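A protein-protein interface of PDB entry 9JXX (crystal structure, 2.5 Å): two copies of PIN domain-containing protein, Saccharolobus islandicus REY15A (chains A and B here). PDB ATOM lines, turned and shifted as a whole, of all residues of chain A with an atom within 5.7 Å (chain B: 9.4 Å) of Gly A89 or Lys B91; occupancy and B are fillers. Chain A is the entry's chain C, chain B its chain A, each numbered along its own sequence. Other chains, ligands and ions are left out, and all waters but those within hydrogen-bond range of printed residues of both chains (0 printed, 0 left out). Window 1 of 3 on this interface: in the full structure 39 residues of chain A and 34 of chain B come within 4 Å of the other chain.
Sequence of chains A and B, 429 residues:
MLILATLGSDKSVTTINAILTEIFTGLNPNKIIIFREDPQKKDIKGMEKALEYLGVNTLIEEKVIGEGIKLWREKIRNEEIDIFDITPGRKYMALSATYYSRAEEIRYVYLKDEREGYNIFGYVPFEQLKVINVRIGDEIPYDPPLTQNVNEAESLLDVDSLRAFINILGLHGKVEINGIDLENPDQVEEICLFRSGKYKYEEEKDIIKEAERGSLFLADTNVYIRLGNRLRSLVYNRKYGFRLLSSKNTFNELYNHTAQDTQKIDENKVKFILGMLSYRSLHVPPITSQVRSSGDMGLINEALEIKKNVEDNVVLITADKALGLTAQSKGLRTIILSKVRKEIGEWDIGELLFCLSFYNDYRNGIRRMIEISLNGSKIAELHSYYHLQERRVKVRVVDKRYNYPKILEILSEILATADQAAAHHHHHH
Of chain B, only Lys B91 comes within 4 Å of Pro A88. Gly A89 touches just one residue of chain B: Lys B91. Of the printed residues of chain B, Tyr A108 touches Lys B91 (3.8 Å). Trp B72 touches none of the printed residues of chain A. Printed residues of chain A within 4 Å of Pro B88: Lys A91 (3.6 Å). Of the printed residues of chain A, Lys B91 touches Ile A86, Thr A87, Pro A88, Gly A89, Arg A90, Ala A94 and Tyr A108. Of the printed residues of chain A, Tyr B108 touches Arg A90 and Lys A91. The nearest printed residue of chain A that does not touch Lys B91 is Lys A91 (4.5 Å).
The backbone carbonyl oxygen (O) of Gly B89 lies within hydrogen-bond range of the side-chain amino group (NZ) of Lys A91 (2.7 Å). NZ of Lys B91 sits at hydrogen-bond distance from O of Pro A88 (3.4 Å). NZ of Lys B91 lies within hydrogen-bond range of O of Thr A87, at 2.7 Å. O of Gly A89 lies within hydrogen-bond range of NZ of Lys B91. NZ of Lys A91 is in hydrogen-bond range of O of Thr B87 (2.8 Å).
The side-chain sulfur (SD) of Met B93 sits at hydrogen-bond distance from the backbone NH (N) of Arg B90, at 3.7 Å. The side-chain carboxylate of Glu B37 is in salt-bridge range of the guanidinium group of Arg B90. The backbone carbonyl oxygen of Ala B94 sits close to the side-chain hydroxyl of Thr B98 (3.4 Å). SD of Met A93 sits at hydrogen-bond distance from N of Arg A90, at 3.3 Å. The backbone carbonyl oxygen (O) of Leu B95 lies within hydrogen-bond range of the side-chain hydroxyl (OG1) of Thr B98 (3.1 Å).
Of the 22 printed residues of chain B, 9 touch a printed residue of chain A. Hydrophobic or aromatic side chains of chain A within 4 Å of the printed part of chain B: Ile A86, Ala A94 and Tyr A108. Among the printed residues, no Asp or Glu carboxylate lies within 4 Å of a Lys or Arg side-chain nitrogen of the other chain.
Pro A88 touches Lys B91, and with the chains exchanged Lys A91 touches Pro B88. Arg A90 touches Lys B91, and with the chains exchanged Lys A91 touches Arg B90. Arg A90 touches Tyr B108, but with the chains exchanged Tyr A108 does not touch Arg B90 (4.1 Å). Lys A91 touches Tyr B108, and with the chains exchanged Tyr A108 touches Lys B91. Positions printed for both chains: 7, 9, 86, 87, 88, 89, 90, 91, 93, 94 and 108. Of the 16 pairs that touch across the chains among the printed residues, 14 have their exchanged pair printed and touching as well.
Ile A86 touches Lys B91 (O to CD, 3.1 Å). Ile A86 touches Leu B95 (CD1 to CD2, 3.8 Å). O of Arg A90 touches CE of Lys B91, at 3.98 Å. OH of Tyr B108 touches CB of Arg A90, at 3.7 Å. Lys A91 touches Ile B86 (CD to O, 3.1 Å). CE of Lys A91 touches O of Pro B88, 3.6 Å away. Lys A91 touches Arg B90 (CE to O, 3.8 Å). Lys A91 touches Tyr B108 (CB to CE1, 3.9 Å). Lys B91 touches Ala A94 (CE to CB, 3.8 Å). Tyr A108 touches Lys B91 (CE1 to CB, 3.8 Å).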
ATOM      1  N   LEU A   7      21.979  17.330 -33.302  1.00  0.00           N
ATOM      2  CA  LEU A   7      21.275  17.967 -32.201  1.00  0.00           C
ATOM      3  C   LEU A   7      22.272  18.479 -31.171  1.00  0.00           C
ATOM      4  O   LEU A   7      23.303  17.845 -30.920  1.00  0.00           O
ATOM      5  CB  LEU A   7      20.289  16.992 -31.550  1.00  0.00           C
ATOM      6  CG  LEU A   7      19.350  16.299 -32.541  1.00  0.00           C
ATOM      7  CD1 LEU A   7      18.738  15.041 -31.944  1.00  0.00           C
ATOM      8  CD2 LEU A   7      18.267  17.259 -33.008  1.00  0.00           C
ATOM      9  N   GLY A   8      21.963  19.632 -30.584  1.00  0.00           N
ATOM     10  CA  GLY A   8      22.841  20.245 -29.609  1.00  0.00           C
ATOM     11  C   GLY A   8      22.420  19.995 -28.179  1.00  0.00           C
ATOM     12  O   GLY A   8      21.447  20.579 -27.693  1.00  0.00           O
ATOM     13  N   SER A   9      23.152  19.125 -27.495  1.00  0.00           N
ATOM     14  CA  SER A   9      22.851  18.801 -26.114  1.00  0.00           C
ATOM     15  C   SER A   9      23.413  19.863 -25.176  1.00  0.00           C
ATOM     16  O   SER A   9      24.240  20.697 -25.555  1.00  0.00           O
ATOM     17  CB  SER A   9      23.421  17.432 -25.754  1.00  0.00           C
ATOM     18  OG  SER A   9      23.352  17.200 -24.359  1.00  0.00           O
ATOM     19  N   THR A  14      28.829  14.979 -26.473  1.00  0.00           N
ATOM     20  CA  THR A  14      28.020  14.114 -27.330  1.00  0.00           C
ATOM     21  C   THR A  14      27.828  14.733 -28.708  1.00  0.00           C
ATOM     22  O   THR A  14      27.977  14.054 -29.729  1.00  0.00           O
ATOM     23  CB  THR A  14      26.666  13.829 -26.682  1.00  0.00           C
ATOM     24  OG1 THR A  14      26.039  15.066 -26.318  1.00  0.00           O
ATOM     25  CG2 THR A  14      26.838  12.962 -25.447  1.00  0.00           C
ATOM     26  N   THR A  15      27.496  16.026 -28.755  1.00  0.00           N
ATOM     27  CA  THR A  15      27.374  16.707 -30.039  1.00  0.00           C
ATOM     28  C   THR A  15      28.703  16.711 -30.783  1.00  0.00           C
ATOM     29  O   THR A  15      28.748  16.460 -31.993  1.00  0.00           O
ATOM     30  CB  THR A  15      26.869  18.137 -29.838  1.00  0.00           C
ATOM     31  OG1 THR A  15      25.557  18.109 -29.263  1.00  0.00           O
ATOM     32  CG2 THR A  15      26.822  18.883 -31.167  1.00  0.00           C
ATOM     33  N   ILE A  86      21.306  11.866 -34.925  1.00  0.00           N
ATOM     34  CA  ILE A  86      20.362  12.117 -33.845  1.00  0.00           C
ATOM     35  C   ILE A  86      20.840  11.521 -32.522  1.00  0.00           C
ATOM     36  O   ILE A  86      20.056  11.386 -31.592  1.00  0.00           O
ATOM     37  CB  ILE A  86      18.956  11.605 -34.209  1.00  0.00           C
ATOM     38  CG1 ILE A  86      19.012  10.131 -34.612  1.00  0.00           C
ATOM     39  CG2 ILE A  86      18.354  12.446 -35.324  1.00  0.00           C
ATOM     40  CD1 ILE A  86      17.941   9.284 -33.961  1.00  0.00           C
ATOM     41  N   THR A  87      22.120  11.161 -32.426  1.00  0.00           N
ATOM     42  CA  THR A  87      22.639  10.616 -31.171  1.00  0.00           C
ATOM     43  C   THR A  87      22.521  11.586 -29.997  1.00  0.00           C
ATOM     44  O   THR A  87      22.042  11.164 -28.931  1.00  0.00           O
ATOM     45  CB  THR A  87      24.089  10.154 -31.362  1.00  0.00           C
ATOM     46  OG1 THR A  87      24.235   9.547 -32.653  1.00  0.00           O
ATOM     47  CG2 THR A  87      24.474   9.149 -30.286  1.00  0.00           C
ATOM     48  N   PRO A  88      22.917  12.856 -30.098  1.00  0.00           N
ATOM     49  CA  PRO A  88      22.832  13.744 -28.935  1.00  0.00           C
ATOM     50  C   PRO A  88      21.406  14.227 -28.697  1.00  0.00           C
ATOM     51  O   PRO A  88      20.502  14.022 -29.506  1.00  0.00           O
ATOM     52  CB  PRO A  88      23.752  14.919 -29.305  1.00  0.00           C
ATOM     53  CG  PRO A  88      24.453  14.509 -30.575  1.00  0.00           C
ATOM     54  CD  PRO A  88      23.528  13.554 -31.242  1.00  0.00           C
ATOM     55  N   GLY A  89      21.220  14.870 -27.545  1.00  0.00           N
ATOM     56  CA  GLY A  89      19.998  15.601 -27.269  1.00  0.00           C
ATOM     57  C   GLY A  89      18.888  14.762 -26.668  1.00  0.00           C
ATOM     58  O   GLY A  89      18.985  13.545 -26.490  1.00  0.00           O
ATOM     59  N   ARG A  90      17.798  15.456 -26.348  1.00  0.00           N
ATOM     60  CA  ARG A  90      16.634  14.823 -25.748  1.00  0.00           C
ATOM     61  C   ARG A  90      15.932  13.919 -26.757  1.00  0.00           C
ATOM     62  O   ARG A  90      16.103  14.042 -27.974  1.00  0.00           O
ATOM     63  CB  ARG A  90      15.661  15.879 -25.221  1.00  0.00           C
ATOM     64  CG  ARG A  90      16.234  16.784 -24.137  1.00  0.00           C
ATOM     65  CD  ARG A  90      15.131  17.598 -23.475  1.00  0.00           C
ATOM     66  NE  ARG A  90      15.639  18.762 -22.758  1.00  0.00           N
ATOM     67  CZ  ARG A  90      15.762  18.833 -21.440  1.00  0.00           C
ATOM     68  NH1 ARG A  90      15.438  17.815 -20.660  1.00  0.00           N
ATOM     69  NH2 ARG A  90      16.220  19.954 -20.890  1.00  0.00           N
ATOM     70  N   LYS A  91      15.125  12.996 -26.229  1.00  0.00           N
ATOM     71  CA  LYS A  91      14.445  12.026 -27.082  1.00  0.00           C
ATOM     72  C   LYS A  91      13.473  12.703 -28.038  1.00  0.00           C
ATOM     73  O   LYS A  91      13.342  12.289 -29.195  1.00  0.00           O
ATOM     74  CB  LYS A  91      13.720  10.992 -26.224  1.00  0.00           C
ATOM     75  CG  LYS A  91      14.632   9.933 -25.639  1.00  0.00           C
ATOM     76  CD  LYS A  91      13.842   8.711 -25.232  1.00  0.00           C
ATOM     77  CE  LYS A  91      14.755   7.550 -24.885  1.00  0.00           C
ATOM     78  NZ  LYS A  91      15.628   7.863 -23.723  1.00  0.00           N
ATOM     79  N   MET A  93      13.755  15.587 -29.370  1.00  0.00           N
ATOM     80  CA  MET A  93      14.505  16.209 -30.456  1.00  0.00           C
ATOM     81  C   MET A  93      14.836  15.196 -31.547  1.00  0.00           C
ATOM     82  O   MET A  93      14.705  15.495 -32.739  1.00  0.00           O
ATOM     83  CB  MET A  93      15.778  16.856 -29.910  1.00  0.00           C
ATOM     84  CG  MET A  93      15.536  17.803 -28.744  1.00  0.00           C
ATOM     85  SD  MET A  93      17.039  18.296 -27.873  1.00  0.00           S
ATOM     86  CE  MET A  93      18.007  19.007 -29.201  1.00  0.00           C
ATOM     87  N   ALA A  94      15.267  13.993 -31.158  1.00  0.00           N
ATOM     88  CA  ALA A  94      15.558  12.956 -32.144  1.00  0.00           C
ATOM     89  C   ALA A  94      14.291  12.498 -32.855  1.00  0.00           C
ATOM     90  O   ALA A  94      14.317  12.225 -34.062  1.00  0.00           O
ATOM     91  CB  ALA A  94      16.259  11.776 -31.473  1.00  0.00           C
ATOM     92  N   TYR A 108      22.671   7.254 -36.498  1.00  0.00           N
ATOM     93  CA  TYR A 108      22.644   7.129 -35.047  1.00  0.00           C
ATOM     94  C   TYR A 108      23.879   6.357 -34.614  1.00  0.00           C
ATOM     95  O   TYR A 108      24.080   5.220 -35.051  1.00  0.00           O
ATOM     96  CB  TYR A 108      21.364   6.419 -34.593  1.00  0.00           C
ATOM     97  CG  TYR A 108      21.402   5.884 -33.180  1.00  0.00           C
ATOM     98  CD1 TYR A 108      21.253   6.732 -32.092  1.00  0.00           C
ATOM     99  CD2 TYR A 108      21.577   4.527 -32.937  1.00  0.00           C
ATOM    100  CE1 TYR A 108      21.282   6.247 -30.799  1.00  0.00           C
ATOM    101  CE2 TYR A 108      21.608   4.031 -31.646  1.00  0.00           C
ATOM    102  CZ  TYR A 108      21.459   4.897 -30.581  1.00  0.00           C
ATOM    103  OH  TYR A 108      21.488   4.417 -29.291  1.00  0.00           O
ATOM    104  N   LEU B   7       9.741   1.418 -21.812  1.00  0.00           N
ATOM    105  CA  LEU B   7      10.993   0.799 -22.219  1.00  0.00           C
ATOM    106  C   LEU B   7      11.831   0.452 -20.996  1.00  0.00           C
ATOM    107  O   LEU B   7      11.864   1.205 -20.017  1.00  0.00           O
ATOM    108  CB  LEU B   7      11.784   1.724 -23.148  1.00  0.00           C
ATOM    109  CG  LEU B   7      11.077   2.121 -24.445  1.00  0.00           C
ATOM    110  CD1 LEU B   7      11.986   2.973 -25.313  1.00  0.00           C
ATOM    111  CD2 LEU B   7      10.615   0.884 -25.198  1.00  0.00           C
ATOM    112  N   SER B   9      15.332   0.227 -19.483  1.00  0.00           N
ATOM    113  CA  SER B   9      16.714   0.654 -19.606  1.00  0.00           C
ATOM    114  C   SER B   9      17.595  -0.097 -18.612  1.00  0.00           C
ATOM    115  O   SER B   9      17.116  -0.844 -17.757  1.00  0.00           O
ATOM    116  CB  SER B   9      16.828   2.161 -19.384  1.00  0.00           C
ATOM    117  OG  SER B   9      17.202   2.449 -18.048  1.00  0.00           O
ATOM    118  N   GLU B  37      15.835  -4.828 -23.820  1.00  0.00           N
ATOM    119  CA  GLU B  37      16.853  -5.224 -24.781  1.00  0.00           C
ATOM    120  C   GLU B  37      17.548  -6.524 -24.405  1.00  0.00           C
ATOM    121  O   GLU B  37      18.218  -7.120 -25.255  1.00  0.00           O
ATOM    122  CB  GLU B  37      17.902  -4.116 -24.923  1.00  0.00           C
ATOM    123  CG  GLU B  37      18.439  -3.924 -26.330  1.00  0.00           C
ATOM    124  CD  GLU B  37      19.741  -3.146 -26.352  1.00  0.00           C
ATOM    125  OE1 GLU B  37      20.635  -3.456 -25.536  1.00  0.00           O
ATOM    126  OE2 GLU B  37      19.871  -2.223 -27.183  1.00  0.00           O
ATOM    127  N   ILE B  69      17.981  -2.732 -34.225  1.00  0.00           N
ATOM    128  CA  ILE B  69      16.795  -1.969 -34.594  1.00  0.00           C
ATOM    129  C   ILE B  69      15.861  -2.795 -35.477  1.00  0.00           C
ATOM    130  O   ILE B  69      14.641  -2.589 -35.460  1.00  0.00           O
ATOM    131  CB  ILE B  69      17.223  -0.654 -35.271  1.00  0.00           C
ATOM    132  CG1 ILE B  69      16.011   0.194 -35.660  1.00  0.00           C
ATOM    133  CG2 ILE B  69      18.102  -0.936 -36.472  1.00  0.00           C
ATOM    134  CD1 ILE B  69      16.331   1.660 -35.802  1.00  0.00           C
ATOM    135  N   TRP B  72      13.503  -4.868 -33.329  1.00  0.00           N
ATOM    136  CA  TRP B  72      12.434  -4.053 -32.764  1.00  0.00           C
ATOM    137  C   TRP B  72      11.393  -3.682 -33.812  1.00  0.00           C
ATOM    138  O   TRP B  72      10.196  -3.641 -33.511  1.00  0.00           O
ATOM    139  CB  TRP B  72      13.023  -2.797 -32.121  1.00  0.00           C
ATOM    140  CG  TRP B  72      13.528  -3.032 -30.734  1.00  0.00           C
ATOM    141  CD1 TRP B  72      14.587  -3.812 -30.369  1.00  0.00           C
ATOM    142  CD2 TRP B  72      12.991  -2.493 -29.520  1.00  0.00           C
ATOM    143  NE1 TRP B  72      14.744  -3.790 -29.005  1.00  0.00           N
ATOM    144  CE2 TRP B  72      13.777  -2.987 -28.461  1.00  0.00           C
ATOM    145  CE3 TRP B  72      11.923  -1.639 -29.228  1.00  0.00           C
ATOM    146  CZ2 TRP B  72      13.529  -2.655 -27.131  1.00  0.00           C
ATOM    147  CZ3 TRP B  72      11.679  -1.311 -27.907  1.00  0.00           C
ATOM    148  CH2 TRP B  72      12.478  -1.818 -26.875  1.00  0.00           C
ATOM    149  N   ILE B  86       7.904   6.448 -23.985  1.00  0.00           N
ATOM    150  CA  ILE B  86       9.208   6.155 -24.559  1.00  0.00           C
ATOM    151  C   ILE B  86      10.329   6.910 -23.844  1.00  0.00           C
ATOM    152  O   ILE B  86      11.441   6.989 -24.359  1.00  0.00           O
ATOM    153  CB  ILE B  86       9.228   6.430 -26.069  1.00  0.00           C
ATOM    154  CG1 ILE B  86       8.397   7.674 -26.411  1.00  0.00           C
ATOM    155  CG2 ILE B  86       8.707   5.223 -26.836  1.00  0.00           C
ATOM    156  CD1 ILE B  86       9.085   8.992 -26.113  1.00  0.00           C
ATOM    157  N   THR B  87      10.052   7.465 -22.662  1.00  0.00           N
ATOM    158  CA  THR B  87      11.070   8.238 -21.954  1.00  0.00           C
ATOM    159  C   THR B  87      12.332   7.442 -21.634  1.00  0.00           C
ATOM    160  O   THR B  87      13.434   7.945 -21.916  1.00  0.00           O
ATOM    161  CB  THR B  87      10.468   8.849 -20.684  1.00  0.00           C
ATOM    162  OG1 THR B  87       9.204   9.451 -20.993  1.00  0.00           O
ATOM    163  CG2 THR B  87      11.400   9.905 -20.109  1.00  0.00           C
ATOM    164  N   PRO B  88      12.273   6.237 -21.068  1.00  0.00           N
ATOM    165  CA  PRO B  88      13.511   5.532 -20.724  1.00  0.00           C
ATOM    166  C   PRO B  88      14.099   4.809 -21.929  1.00  0.00           C
ATOM    167  O   PRO B  88      13.502   4.732 -23.004  1.00  0.00           O
ATOM    168  CB  PRO B  88      13.074   4.536 -19.638  1.00  0.00           C
ATOM    169  CG  PRO B  88      11.563   4.573 -19.609  1.00  0.00           C
ATOM    170  CD  PRO B  88      11.091   5.417 -20.747  1.00  0.00           C
ATOM    171  N   GLY B  89      15.308   4.284 -21.730  1.00  0.00           N
ATOM    172  CA  GLY B  89      15.944   3.436 -22.718  1.00  0.00           C
ATOM    173  C   GLY B  89      16.745   4.196 -23.755  1.00  0.00           C
ATOM    174  O   GLY B  89      16.841   5.426 -23.761  1.00  0.00           O
ATOM    175  N   ARG B  90      17.340   3.421 -24.660  1.00  0.00           N
ATOM    176  CA  ARG B  90      18.137   3.988 -25.736  1.00  0.00           C
ATOM    177  C   ARG B  90      17.244   4.717 -26.734  1.00  0.00           C
ATOM    178  O   ARG B  90      16.028   4.517 -26.788  1.00  0.00           O
ATOM    179  CB  ARG B  90      18.930   2.898 -26.458  1.00  0.00           C
ATOM    180  CG  ARG B  90      19.742   1.992 -25.549  1.00  0.00           C
ATOM    181  CD  ARG B  90      20.411   0.899 -26.364  1.00  0.00           C
ATOM    182  NE  ARG B  90      21.283   0.046 -25.567  1.00  0.00           N
ATOM    183  CZ  ARG B  90      22.599   0.189 -25.488  1.00  0.00           C
ATOM    184  NH1 ARG B  90      23.228   1.161 -26.129  1.00  0.00           N
ATOM    185  NH2 ARG B  90      23.302  -0.666 -24.752  1.00  0.00           N
ATOM    186  N   LYS B  91      17.873   5.577 -27.537  1.00  0.00           N
ATOM    187  CA  LYS B  91      17.118   6.352 -28.513  1.00  0.00           C
ATOM    188  C   LYS B  91      16.454   5.445 -29.543  1.00  0.00           C
ATOM    189  O   LYS B  91      15.248   5.551 -29.788  1.00  0.00           O
ATOM    190  CB  LYS B  91      18.033   7.375 -29.188  1.00  0.00           C
ATOM    191  CG  LYS B  91      18.020   8.732 -28.504  1.00  0.00           C
ATOM    192  CD  LYS B  91      18.813   9.757 -29.284  1.00  0.00           C
ATOM    193  CE  LYS B  91      18.739  11.130 -28.635  1.00  0.00           C
ATOM    194  NZ  LYS B  91      19.768  11.303 -27.571  1.00  0.00           N
ATOM    195  N   TYR B  92      17.218   4.513 -30.126  1.00  0.00           N
ATOM    196  CA  TYR B  92      16.665   3.663 -31.179  1.00  0.00           C
ATOM    197  C   TYR B  92      15.488   2.840 -30.668  1.00  0.00           C
ATOM    198  O   TYR B  92      14.532   2.585 -31.409  1.00  0.00           O
ATOM    199  CB  TYR B  92      17.756   2.762 -31.766  1.00  0.00           C
ATOM    200  CG  TYR B  92      17.950   1.429 -31.069  1.00  0.00           C
ATOM    201  CD1 TYR B  92      17.238   0.301 -31.465  1.00  0.00           C
ATOM    202  CD2 TYR B  92      18.861   1.295 -30.030  1.00  0.00           C
ATOM    203  CE1 TYR B  92      17.417  -0.916 -30.834  1.00  0.00           C
ATOM    204  CE2 TYR B  92      19.046   0.080 -29.397  1.00  0.00           C
ATOM    205  CZ  TYR B  92      18.322  -1.020 -29.801  1.00  0.00           C
ATOM    206  OH  TYR B  92      18.506  -2.230 -29.171  1.00  0.00           O
ATOM    207  N   MET B  93      15.537   2.418 -29.402  1.00  0.00           N
ATOM    208  CA  MET B  93      14.389   1.735 -28.811  1.00  0.00           C
ATOM    209  C   MET B  93      13.170   2.646 -28.790  1.00  0.00           C
ATOM    210  O   MET B  93      12.054   2.213 -29.101  1.00  0.00           O
ATOM    211  CB  MET B  93      14.728   1.259 -27.399  1.00  0.00           C
ATOM    212  CG  MET B  93      15.762   0.146 -27.340  1.00  0.00           C
ATOM    213  SD  MET B  93      16.445  -0.069 -25.683  1.00  0.00           S
ATOM    214  CE  MET B  93      14.945  -0.232 -24.717  1.00  0.00           C
ATOM    215  N   ALA B  94      13.365   3.916 -28.429  1.00  0.00           N
ATOM    216  CA  ALA B  94      12.273   4.879 -28.498  1.00  0.00           C
ATOM    217  C   ALA B  94      11.885   5.183 -29.938  1.00  0.00           C
ATOM    218  O   ALA B  94      10.711   5.438 -30.219  1.00  0.00           O
ATOM    219  CB  ALA B  94      12.655   6.167 -27.768  1.00  0.00           C
ATOM    220  N   LEU B  95      12.850   5.167 -30.861  1.00  0.00           N
ATOM    221  CA  LEU B  95      12.547   5.479 -32.257  1.00  0.00           C
ATOM    222  C   LEU B  95      11.571   4.469 -32.853  1.00  0.00           C
ATOM    223  O   LEU B  95      10.542   4.845 -33.426  1.00  0.00           O
ATOM    224  CB  LEU B  95      13.837   5.532 -33.079  1.00  0.00           C
ATOM    225  CG  LEU B  95      14.475   6.900 -33.350  1.00  0.00           C
ATOM    226  CD1 LEU B  95      13.457   7.833 -33.976  1.00  0.00           C
ATOM    227  CD2 LEU B  95      15.088   7.534 -32.111  1.00  0.00           C
ATOM    228  N   SER B  96      11.877   3.175 -32.725  1.00  0.00           N
ATOM    229  CA  SER B  96      11.016   2.152 -33.309  1.00  0.00           C
ATOM    230  C   SER B  96       9.681   2.053 -32.583  1.00  0.00           C
ATOM    231  O   SER B  96       8.659   1.748 -33.209  1.00  0.00           O
ATOM    232  CB  SER B  96      11.726   0.798 -33.301  1.00  0.00           C
ATOM    233  OG  SER B  96      12.144   0.448 -31.994  1.00  0.00           O
ATOM    234  N   ALA B  97       9.668   2.304 -31.271  1.00  0.00           N
ATOM    235  CA  ALA B  97       8.429   2.205 -30.508  1.00  0.00           C
ATOM    236  C   ALA B  97       7.418   3.270 -30.920  1.00  0.00           C
ATOM    237  O   ALA B  97       6.211   3.008 -30.913  1.00  0.00           O
ATOM    238  CB  ALA B  97       8.722   2.301 -29.012  1.00  0.00           C
ATOM    239  N   THR B  98       7.878   4.465 -31.280  1.00  0.00           N
ATOM    240  CA  THR B  98       6.968   5.521 -31.711  1.00  0.00           C
ATOM    241  C   THR B  98       6.549   5.389 -33.168  1.00  0.00           C
ATOM    242  O   THR B  98       5.718   6.181 -33.626  1.00  0.00           O
ATOM    243  CB  THR B  98       7.599   6.900 -31.492  1.00  0.00           C
ATOM    244  OG1 THR B  98       8.664   7.097 -32.431  1.00  0.00           O
ATOM    245  CG2 THR B  98       8.140   7.023 -30.082  1.00  0.00           C
ATOM    246  N   TYR B  99       7.095   4.420 -33.906  1.00  0.00           N
ATOM    247  CA  TYR B  99       6.782   4.268 -35.318  1.00  0.00           C
ATOM    248  C   TYR B  99       6.238   2.899 -35.701  1.00  0.00           C
ATOM    249  O   TYR B  99       5.623   2.783 -36.766  1.00  0.00           O
ATOM    250  CB  TYR B  99       8.024   4.560 -36.177  1.00  0.00           C
ATOM    251  CG  TYR B  99       7.698   4.922 -37.610  1.00  0.00           C
ATOM    252  CD1 TYR B  99       6.646   5.777 -37.906  1.00  0.00           C
ATOM    253  CD2 TYR B  99       8.441   4.409 -38.663  1.00  0.00           C
ATOM    254  CE1 TYR B  99       6.340   6.110 -39.212  1.00  0.00           C
ATOM    255  CE2 TYR B  99       8.144   4.735 -39.974  1.00  0.00           C
ATOM    256  CZ  TYR B  99       7.093   5.586 -40.243  1.00  0.00           C
ATOM    257  OH  TYR B  99       6.794   5.914 -41.545  1.00  0.00           O
ATOM    258  N   TYR B 108       5.954  11.244 -23.536  1.00  0.00           N
ATOM    259  CA  TYR B 108       7.329  11.541 -23.155  1.00  0.00           C
ATOM    260  C   TYR B 108       7.309  12.391 -21.894  1.00  0.00           C
ATOM    261  O   TYR B 108       6.624  13.417 -21.850  1.00  0.00           O
ATOM    262  CB  TYR B 108       8.060  12.271 -24.290  1.00  0.00           C
ATOM    263  CG  TYR B 108       9.425  12.811 -23.925  1.00  0.00           C
ATOM    264  CD1 TYR B 108      10.467  11.957 -23.588  1.00  0.00           C
ATOM    265  CD2 TYR B 108       9.675  14.179 -23.927  1.00  0.00           C
ATOM    266  CE1 TYR B 108      11.717  12.448 -23.258  1.00  0.00           C
ATOM    267  CE2 TYR B 108      10.922  14.680 -23.599  1.00  0.00           C
ATOM    268  CZ  TYR B 108      11.940  13.810 -23.265  1.00  0.00           C
ATOM    269  OH  TYR B 108      13.184  14.299 -22.936  1.00  0.00           O
ATOM    270  N   GLU B 114      17.793  18.192 -16.432  1.00  0.00           N
ATOM    271  CA  GLU B 114      18.121  16.783 -16.245  1.00  0.00           C
ATOM    272  C   GLU B 114      19.009  16.543 -15.030  1.00  0.00           C
ATOM    273  O   GLU B 114      19.032  15.424 -14.506  1.00  0.00           O
ATOM    274  CB  GLU B 114      18.790  16.241 -17.510  1.00  0.00           C
ATOM    275  CG  GLU B 114      19.106  14.756 -17.491  1.00  0.00           C
ATOM    276  CD  GLU B 114      19.954  14.344 -18.671  1.00  0.00           C
ATOM    277  OE1 GLU B 114      20.174  15.198 -19.552  1.00  0.00           O
ATOM    278  OE2 GLU B 114      20.402  13.180 -18.719  1.00  0.00           O
ATOM    279  N   TYR B 118      17.029  11.150 -12.302  1.00  0.00           N
ATOM    280  CA  TYR B 118      17.606   9.888 -11.837  1.00  0.00           C
ATOM    281  C   TYR B 118      17.538   9.757 -10.318  1.00  0.00           C
ATOM    282  O   TYR B 118      18.381   9.105  -9.698  1.00  0.00           O
ATOM    283  CB  TYR B 118      19.043   9.727 -12.345  1.00  0.00           C
ATOM    284  CG  TYR B 118      19.161  10.024 -13.824  1.00  0.00           C
ATOM    285  CD1 TYR B 118      18.866   9.054 -14.771  1.00  0.00           C
ATOM    286  CD2 TYR B 118      19.536  11.285 -14.274  1.00  0.00           C
ATOM    287  CE1 TYR B 118      18.957   9.323 -16.123  1.00  0.00           C
ATOM    288  CE2 TYR B 118      19.626  11.564 -15.625  1.00  0.00           C
ATOM    289  CZ  TYR B 118      19.337  10.579 -16.545  1.00  0.00           C
ATOM    290  OH  TYR B 118      19.427  10.849 -17.891  1.00  0.00           O
